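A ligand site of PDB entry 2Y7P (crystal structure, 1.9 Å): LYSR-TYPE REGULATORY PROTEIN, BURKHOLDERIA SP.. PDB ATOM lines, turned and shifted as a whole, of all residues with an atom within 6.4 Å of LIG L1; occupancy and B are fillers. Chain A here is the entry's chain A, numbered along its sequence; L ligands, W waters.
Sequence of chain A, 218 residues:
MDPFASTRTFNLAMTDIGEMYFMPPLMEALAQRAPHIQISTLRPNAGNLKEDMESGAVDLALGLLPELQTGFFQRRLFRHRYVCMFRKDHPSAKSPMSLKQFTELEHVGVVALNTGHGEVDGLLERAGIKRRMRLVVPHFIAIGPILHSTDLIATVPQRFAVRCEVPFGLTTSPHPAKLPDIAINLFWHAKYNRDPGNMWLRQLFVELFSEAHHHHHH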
ATOM      1  N   MET A  14      18.140  21.087  10.162  1.00  0.00           N
ATOM      2  CA  MET A  14      17.007  22.022  10.349  1.00  0.00           C
ATOM      3  C   MET A  14      17.465  23.084  11.362  1.00  0.00           C
ATOM      4  O   MET A  14      18.422  22.864  12.118  1.00  0.00           O
ATOM      5  CB  MET A  14      15.745  21.298  10.878  1.00  0.00           C
ATOM      6  CG  MET A  14      15.940  20.681  12.305  1.00  0.00           C
ATOM      7  SD  MET A  14      14.666  19.468  12.655  1.00  0.00           S
ATOM      8  CE  MET A  14      15.195  18.137  11.569  1.00  0.00           C
ATOM      9  N   THR A  15      16.752  24.210  11.413  1.00  0.00           N
ATOM     10  CA  THR A  15      17.117  25.323  12.314  1.00  0.00           C
ATOM     11  C   THR A  15      16.624  25.003  13.725  1.00  0.00           C
ATOM     12  O   THR A  15      15.928  23.963  13.973  1.00  0.00           O
ATOM     13  CB  THR A  15      16.463  26.639  11.852  1.00  0.00           C
ATOM     14  OG1 THR A  15      15.041  26.468  11.908  1.00  0.00           O
ATOM     15  CG2 THR A  15      16.899  27.004  10.397  1.00  0.00           C
ATOM     16  N   ILE A  17      14.247  26.612  15.331  1.00  0.00           N
ATOM     17  CA  ILE A  17      12.775  26.675  15.142  1.00  0.00           C
ATOM     18  C   ILE A  17      12.258  25.373  14.549  1.00  0.00           C
ATOM     19  O   ILE A  17      11.217  24.801  14.972  1.00  0.00           O
ATOM     20  CB  ILE A  17      12.404  27.816  14.121  1.00  0.00           C
ATOM     21  CG1 ILE A  17      12.623  29.193  14.728  1.00  0.00           C
ATOM     22  CG2 ILE A  17      10.952  27.716  13.647  1.00  0.00           C
ATOM     23  CD1 ILE A  17      12.192  30.292  13.756  1.00  0.00           C
ATOM     24  N   GLY A  18      12.969  24.931  13.501  1.00  0.00           N
ATOM     25  CA  GLY A  18      12.596  23.686  12.819  1.00  0.00           C
ATOM     26  C   GLY A  18      12.632  22.490  13.786  1.00  0.00           C
ATOM     27  O   GLY A  18      11.736  21.656  13.808  1.00  0.00           O
ATOM     28  N   GLU A  19      13.653  22.455  14.645  1.00  0.00           N
ATOM     29  CA  GLU A  19      13.801  21.353  15.614  1.00  0.00           C
ATOM     30  C   GLU A  19      12.602  21.303  16.595  1.00  0.00           C
ATOM     31  O   GLU A  19      12.022  20.215  16.861  1.00  0.00           O
ATOM     32  CB  GLU A  19      15.156  21.525  16.344  1.00  0.00           C
ATOM     33  CG  GLU A  19      15.624  20.265  17.063  1.00  0.00           C
ATOM     34  CD  GLU A  19      17.099  20.324  17.302  1.00  0.00           C
ATOM     35  OE1 GLU A  19      17.905  19.971  16.412  1.00  0.00           O
ATOM     36  OE2 GLU A  19      17.436  20.788  18.387  1.00  0.00           O
ATOM     37  N   TYR A  21       9.653  22.583  16.044  1.00  0.00           N
ATOM     38  CA  TYR A  21       8.414  22.320  15.262  1.00  0.00           C
ATOM     39  C   TYR A  21       8.294  20.877  14.787  1.00  0.00           C
ATOM     40  O   TYR A  21       7.238  20.242  14.947  1.00  0.00           O
ATOM     41  CB  TYR A  21       8.448  23.297  14.052  1.00  0.00           C
ATOM     42  CG  TYR A  21       7.147  23.295  13.247  1.00  0.00           C
ATOM     43  CD1 TYR A  21       6.068  24.100  13.640  1.00  0.00           C
ATOM     44  CD2 TYR A  21       7.012  22.506  12.116  1.00  0.00           C
ATOM     45  CE1 TYR A  21       4.869  24.106  12.902  1.00  0.00           C
ATOM     46  CE2 TYR A  21       5.801  22.496  11.363  1.00  0.00           C
ATOM     47  CZ  TYR A  21       4.747  23.284  11.763  1.00  0.00           C
ATOM     48  OH  TYR A  21       3.593  23.287  11.003  1.00  0.00           O
ATOM     49  N   PHE A  22       9.351  20.352  14.187  1.00  0.00           N
ATOM     50  CA  PHE A  22       9.321  19.030  13.471  1.00  0.00           C
ATOM     51  C   PHE A  22       9.596  17.822  14.374  1.00  0.00           C
ATOM     52  O   PHE A  22       9.000  16.736  14.184  1.00  0.00           O
ATOM     53  CB  PHE A  22      10.339  19.007  12.338  1.00  0.00           C
ATOM     54  CG  PHE A  22       9.993  19.911  11.195  1.00  0.00           C
ATOM     55  CD1 PHE A  22       8.792  19.726  10.484  1.00  0.00           C
ATOM     56  CD2 PHE A  22      10.848  20.981  10.864  1.00  0.00           C
ATOM     57  CE1 PHE A  22       8.408  20.578   9.417  1.00  0.00           C
ATOM     58  CE2 PHE A  22      10.514  21.837   9.764  1.00  0.00           C
ATOM     59  CZ  PHE A  22       9.273  21.655   9.041  1.00  0.00           C
ATOM     60  N   LEU A  62      15.268  20.508   6.135  1.00  0.00           N
ATOM     61  CA  LEU A  62      13.938  21.160   6.278  1.00  0.00           C
ATOM     62  C   LEU A  62      14.151  22.634   6.526  1.00  0.00           C
ATOM     63  O   LEU A  62      14.951  23.000   7.412  1.00  0.00           O
ATOM     64  CB  LEU A  62      13.234  20.582   7.525  1.00  0.00           C
ATOM     65  CG  LEU A  62      12.823  19.180   7.088  1.00  0.00           C
ATOM     66  CD1 LEU A  62      13.679  18.069   7.712  1.00  0.00           C
ATOM     67  CD2 LEU A  62      11.359  18.985   7.079  1.00  0.00           C
ATOM     68  N   GLY A  63      13.389  23.487   5.860  1.00  0.00           N
ATOM     69  CA  GLY A  63      13.469  24.941   6.180  1.00  0.00           C
ATOM     70  C   GLY A  63      13.402  25.827   4.939  1.00  0.00           C
ATOM     71  O   GLY A  63      12.842  25.409   3.894  1.00  0.00           O
ATOM     72  N   LEU A  64      13.952  27.038   5.069  1.00  0.00           N
ATOM     73  CA  LEU A  64      14.012  28.010   3.970  1.00  0.00           C
ATOM     74  C   LEU A  64      15.450  27.918   3.477  1.00  0.00           C
ATOM     75  O   LEU A  64      16.352  28.469   4.088  1.00  0.00           O
ATOM     76  CB  LEU A  64      13.695  29.413   4.495  1.00  0.00           C
ATOM     77  CG  LEU A  64      13.815  30.582   3.505  1.00  0.00           C
ATOM     78  CD1 LEU A  64      12.715  30.457   2.327  1.00  0.00           C
ATOM     79  CD2 LEU A  64      13.594  31.896   4.225  1.00  0.00           C
ATOM     80  N   PHE A  78       4.668  24.080   3.850  1.00  0.00           N
ATOM     81  CA  PHE A  78       3.721  25.212   3.980  1.00  0.00           C
ATOM     82  C   PHE A  78       4.515  26.479   3.656  1.00  0.00           C
ATOM     83  O   PHE A  78       5.756  26.406   3.507  1.00  0.00           O
ATOM     84  CB  PHE A  78       3.095  25.301   5.419  1.00  0.00           C
ATOM     85  CG  PHE A  78       4.138  25.258   6.516  1.00  0.00           C
ATOM     86  CD1 PHE A  78       4.586  24.036   7.026  1.00  0.00           C
ATOM     87  CD2 PHE A  78       4.705  26.444   6.992  1.00  0.00           C
ATOM     88  CE1 PHE A  78       5.607  23.993   8.028  1.00  0.00           C
ATOM     89  CE2 PHE A  78       5.694  26.404   8.012  1.00  0.00           C
ATOM     90  CZ  PHE A  78       6.111  25.187   8.514  1.00  0.00           C
ATOM     91  N   HIS A  80       4.699  30.956   4.697  1.00  0.00           N
ATOM     92  CA  HIS A  80       4.240  31.993   5.666  1.00  0.00           C
ATOM     93  C   HIS A  80       5.076  33.231   5.407  1.00  0.00           C
ATOM     94  O   HIS A  80       5.922  33.214   4.506  1.00  0.00           O
ATOM     95  CB  HIS A  80       4.193  31.477   7.143  1.00  0.00           C
ATOM     96  CG  HIS A  80       5.528  31.036   7.699  1.00  0.00           C
ATOM     97  ND1 HIS A  80       5.877  31.273   9.028  1.00  0.00           N
ATOM     98  CD2 HIS A  80       6.554  30.327   7.157  1.00  0.00           C
ATOM     99  CE1 HIS A  80       7.075  30.720   9.268  1.00  0.00           C
ATOM    100  NE2 HIS A  80       7.506  30.152   8.156  1.00  0.00           N
ATOM    101  N   THR A 115      20.751  30.161   6.051  1.00  0.00           N
ATOM    102  CA  THR A 115      19.372  29.935   5.557  1.00  0.00           C
ATOM    103  C   THR A 115      18.902  31.171   4.762  1.00  0.00           C
ATOM    104  O   THR A 115      19.581  32.185   4.770  1.00  0.00           O
ATOM    105  CB  THR A 115      18.397  29.761   6.721  1.00  0.00           C
ATOM    106  OG1 THR A 115      18.289  31.016   7.426  1.00  0.00           O
ATOM    107  CG2 THR A 115      18.881  28.613   7.724  1.00  0.00           C
ATOM    108  N   HIS A 117      16.725  33.124   5.609  1.00  0.00           N
ATOM    109  CA  HIS A 117      16.443  34.233   6.528  1.00  0.00           C
ATOM    110  C   HIS A 117      17.639  35.172   6.632  1.00  0.00           C
ATOM    111  O   HIS A 117      17.504  36.342   7.040  1.00  0.00           O
ATOM    112  CB  HIS A 117      16.093  33.705   7.911  1.00  0.00           C
ATOM    113  CG  HIS A 117      14.926  32.741   7.922  1.00  0.00           C
ATOM    114  ND1 HIS A 117      13.621  33.123   7.635  1.00  0.00           N
ATOM    115  CD2 HIS A 117      14.867  31.422   8.259  1.00  0.00           C
ATOM    116  CE1 HIS A 117      12.813  32.084   7.784  1.00  0.00           C
ATOM    117  NE2 HIS A 117      13.540  31.030   8.157  1.00  0.00           N
ATOM    118  N   PHE A 140      16.943  32.713  15.741  1.00  0.00           N
ATOM    119  CA  PHE A 140      15.660  33.262  16.208  1.00  0.00           C
ATOM    120  C   PHE A 140      15.231  32.872  17.615  1.00  0.00           C
ATOM    121  O   PHE A 140      14.475  33.611  18.218  1.00  0.00           O
ATOM    122  CB  PHE A 140      14.523  32.860  15.262  1.00  0.00           C
ATOM    123  CG  PHE A 140      14.511  33.637  13.963  1.00  0.00           C
ATOM    124  CD1 PHE A 140      14.121  34.988  13.944  1.00  0.00           C
ATOM    125  CD2 PHE A 140      14.857  33.016  12.771  1.00  0.00           C
ATOM    126  CE1 PHE A 140      14.115  35.740  12.762  1.00  0.00           C
ATOM    127  CE2 PHE A 140      14.834  33.759  11.534  1.00  0.00           C
ATOM    128  CZ  PHE A 140      14.455  35.135  11.527  1.00  0.00           C
ATOM    129  N   PRO A 157       9.678  35.125  11.355  1.00  0.00           N
ATOM    130  CA  PRO A 157       8.693  34.282  10.636  1.00  0.00           C
ATOM    131  C   PRO A 157       7.357  34.216  11.370  1.00  0.00           C
ATOM    132  O   PRO A 157       7.325  34.021  12.592  1.00  0.00           O
ATOM    133  CB  PRO A 157       9.355  32.899  10.650  1.00  0.00           C
ATOM    134  CG  PRO A 157      10.860  33.197  10.642  1.00  0.00           C
ATOM    135  CD  PRO A 157      10.919  34.362  11.652  1.00  0.00           C
ATOM    136  N   GLN A 158       6.245  34.356  10.667  1.00  0.00           N
ATOM    137  CA  GLN A 158       4.941  34.452  11.373  1.00  0.00           C
ATOM    138  C   GLN A 158       4.596  33.246  12.238  1.00  0.00           C
ATOM    139  O   GLN A 158       4.148  33.425  13.386  1.00  0.00           O
ATOM    140  CB  GLN A 158       3.799  34.808  10.396  1.00  0.00           C
ATOM    141  CG  GLN A 158       2.379  34.799  10.996  1.00  0.00           C
ATOM    142  CD  GLN A 158       1.656  33.462  10.745  1.00  0.00           C
ATOM    143  OE1 GLN A 158       0.939  32.962  11.610  1.00  0.00           O
ATOM    144  NE2 GLN A 158       1.798  32.913   9.538  1.00  0.00           N
ATOM    145  N   ARG A 159       4.805  31.998  11.763  1.00  0.00           N
ATOM    146  CA  ARG A 159       4.440  30.874  12.629  1.00  0.00           C
ATOM    147  C   ARG A 159       5.225  30.784  13.971  1.00  0.00           C
ATOM    148  O   ARG A 159       4.712  30.248  14.972  1.00  0.00           O
ATOM    149  CB  ARG A 159       4.543  29.520  11.912  1.00  0.00           C
ATOM    150  CG  ARG A 159       3.484  29.378  10.868  1.00  0.00           C
ATOM    151  CD  ARG A 159       3.420  27.963  10.334  1.00  0.00           C
ATOM    152  NE  ARG A 159       2.329  27.929   9.373  1.00  0.00           N
ATOM    153  CZ  ARG A 159       1.778  26.816   8.921  1.00  0.00           C
ATOM    154  NH1 ARG A 159       2.235  25.606   9.338  1.00  0.00           N
ATOM    155  NH2 ARG A 159       0.767  26.944   8.089  1.00  0.00           N
ATOM    156  N   PHE A 160       6.481  31.232  13.936  1.00  0.00           N
ATOM    157  CA  PHE A 160       7.277  31.288  15.140  1.00  0.00           C
ATOM    158  C   PHE A 160       6.750  32.438  16.052  1.00  0.00           C
ATOM    159  O   PHE A 160       6.551  32.205  17.263  1.00  0.00           O
ATOM    160  CB  PHE A 160       8.727  31.525  14.788  1.00  0.00           C
ATOM    161  CG  PHE A 160       9.594  31.756  15.995  1.00  0.00           C
ATOM    162  CD1 PHE A 160       9.696  30.780  16.975  1.00  0.00           C
ATOM    163  CD2 PHE A 160      10.271  32.935  16.158  1.00  0.00           C
ATOM    164  CE1 PHE A 160      10.492  31.000  18.098  1.00  0.00           C
ATOM    165  CE2 PHE A 160      11.072  33.157  17.319  1.00  0.00           C
ATOM    166  CZ  PHE A 160      11.171  32.172  18.240  1.00  0.00           C
ATOM    167  N   ILE A 182       8.137  33.025   2.873  1.00  0.00           N
ATOM    168  CA  ILE A 182       8.964  31.995   3.494  1.00  0.00           C
ATOM    169  C   ILE A 182       8.391  30.650   3.081  1.00  0.00           C
ATOM    170  O   ILE A 182       7.381  30.176   3.671  1.00  0.00           O
ATOM    171  CB  ILE A 182       9.008  32.105   5.064  1.00  0.00           C
ATOM    172  CG1 ILE A 182       9.575  33.468   5.504  1.00  0.00           C
ATOM    173  CG2 ILE A 182       9.935  30.960   5.631  1.00  0.00           C
ATOM    174  CD1 ILE A 182       9.165  33.863   7.027  1.00  0.00           C
ATOM    175  N   ILE A 184       8.609  26.863   3.323  1.00  0.00           N
ATOM    176  CA  ILE A 184       9.228  25.843   4.131  1.00  0.00           C
ATOM    177  C   ILE A 184       9.073  24.511   3.418  1.00  0.00           C
ATOM    178  O   ILE A 184       7.966  24.013   3.291  1.00  0.00           O
ATOM    179  CB  ILE A 184       8.621  25.757   5.545  1.00  0.00           C
ATOM    180  CG1 ILE A 184       8.794  27.132   6.292  1.00  0.00           C
ATOM    181  CG2 ILE A 184       9.353  24.659   6.344  1.00  0.00           C
ATOM    182  CD1 ILE A 184      10.317  27.584   6.499  1.00  0.00           C
HETATM  183  C1  LIG L   1      12.258  27.611   9.581  1.00  0.00           C
HETATM  184  O1  LIG L   1      13.296  26.896   9.482  1.00  0.00           O
HETATM  185  O2  LIG L   1      12.288  28.839   9.300  1.00  0.00           O
HETATM  186  C2  LIG L   1      10.973  27.056  10.052  1.00  0.00           C
HETATM  187  C3  LIG L   1       9.804  27.946  10.172  1.00  0.00           C
HETATM  188  C4  LIG L   1       8.605  27.433  10.656  1.00  0.00           C
HETATM  189  C5  LIG L   1       8.491  26.080  11.029  1.00  0.00           C
HETATM  190  C6  LIG L   1       9.605  25.262  10.918  1.00  0.00           C
HETATM  191  C7  LIG L   1      10.853  25.714  10.431  1.00  0.00           C
HETATM  192  O3  LIG L   1       9.918  29.250   9.776  1.00  0.00           O
HETATM  193  O1  LG2 L   2       7.018  27.687  14.431  1.00  0.00           O
HETATM  194  C1  LG2 L   2       8.071  27.112  15.301  1.00  0.00           C
HETATM  195  C2  LG2 L   2       7.851  27.005  16.819  1.00  0.00           C
HETATM  196  O2  LG2 L   2       7.377  25.755  17.411  1.00  0.00           O
HETATM  197  C3  LG2 L   2       7.465  25.779  18.865  1.00  0.00           C
HETATM  198  C4  LG2 L   2       6.801  24.496  19.466  1.00  0.00           C
HETATM  199  O3  LG2 L   2       6.137  24.722  20.753  1.00  0.00           O
HETATM  200  C5  LG2 L   2       6.200  23.568  21.712  1.00  0.00           C
HETATM  201  C6  LG2 L   2       4.930  22.779  22.172  1.00  0.00           C
HETATM  202  O4  LG2 L   2       5.046  22.157  23.533  1.00  0.00           O
HETATM  203  C7  LG2 L   2       3.818  21.548  24.121  1.00  0.00           C
HETATM  204  C8  LG2 L   2       2.860  22.498  24.942  1.00  0.00           C
HETATM  205  O5  LG2 L   2       3.116  23.888  24.449  1.00  0.00           O
HETATM  206  C9  LG2 L   2       2.464  24.990  25.175  1.00  0.00           C
HETATM  207  C10 LG2 L   2       3.149  26.331  24.781  1.00  0.00           C
HETATM  208  O6  LG2 L   2       4.389  26.694  25.513  1.00  0.00           O
HETATM  209  C11 LG2 L   2       5.516  26.856  24.603  1.00  0.00           C
HETATM  210  C12 LG2 L   2       6.321  28.178  24.786  1.00  0.00           C
HETATM  211  O7  LG2 L   2       7.571  28.378  23.933  1.00  0.00           O
HETATM  212  C13 LG2 L   2       7.410  28.469  22.432  1.00  0.00           C
HETATM  213  C14 LG2 L   2       8.636  29.052  21.698  1.00  0.00           C
HETATM  214  O8  LG2 L   2       9.702  28.952  22.705  1.00  0.00           O
HETATM  215  C15 LG2 L   2      11.080  29.142  22.221  1.00  0.00           C
HETATM  216  O   HOH W   1      14.194  24.335   9.769  1.00  0.00           O
HETATM  217  O   HOH W   2      15.005  27.743   7.662  1.00  0.00           O
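The backbone NH (N) of His 117 lies close to the side-chain hydroxyl (OG1) of Thr 115, 3.2 Å away. The side-chain hydroxyl of Thr 15 is in hydrogen-bond range of the backbone NH of Gly 18, at 3.0 Å. The backbone carbonyl oxygen (O) of His 80 is in hydrogen-bond range of the backbone NH (N) of Ile 182 (2.8 Å). The backbone NH (N) of Arg 159 sits at hydrogen-bond distance from a ring nitrogen (ND1) of His 80 (3.0 Å). The backbone carbonyl oxygen (O) of Phe 78 sits at hydrogen-bond distance from the backbone NH (N) of Ile 184 (2.9 Å). The side-chain hydroxyl of Tyr 21 lies within hydrogen-bond range of the guanidinium group of Arg 159, at 3.2 Å.
CG2 of Ile 17 touches C2 of LIG L1, at 3.7 Å. CA of Gly 18 touches C7 of LIG L1, at 3.6 Å. Tyr 21 touches LIG L1. Phe 22 touches LIG L1 (CE2 to C6, 3.7 Å). Gly 63 touches LIG L1 (CA to O1, 3.8 Å). Phe 78 touches LIG L1 (CZ to C5, 3.6 Å). CB of Pro 157 touches O3 of LIG L1, 3.8 Å away. Ile 184 touches LIG L1 (CD1 to C1, 3.6 Å). Hydrophobic or aromatic side chains that line LIG L1: Ile 17, Tyr 21, Phe 22, Phe 78, His 80, His 117, Pro 157 and Ile 184. 11 residues have an atom within 4 Å of LIG L1: Thr 15, Ile 17, Gly 18, Tyr 21, Phe 22, Gly 63, Phe 78, His 80, His 117, Pro 157 and Ile 184. The nearest printed residue that does not touch LIG L1 is Leu 64 (4.5 Å).
An oxygen (O2) of LIG L1 lies within hydrogen-bond range of a ring nitrogen (NE2) of His 117. The side-chain hydroxyl of Thr 15 is in hydrogen-bond range of an oxygen (O1) of LIG L1, at 3.0 Å. A ring nitrogen (NE2) of His 80 is in hydrogen-bond range of an oxygen (O3) of LIG L1 (3.0 Å).
Water W2 lies within hydrogen-bond range of O1 of LIG L1 (2.6 Å) and N of Leu 64 (2.9 Å). Water W1 lies within hydrogen-bond range of an oxygen (O1) of LIG L1 (2.7 Å), the backbone carbonyl oxygen of Leu 62 (2.8 Å) and the backbone NH of Thr 15 (3.0 Å).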
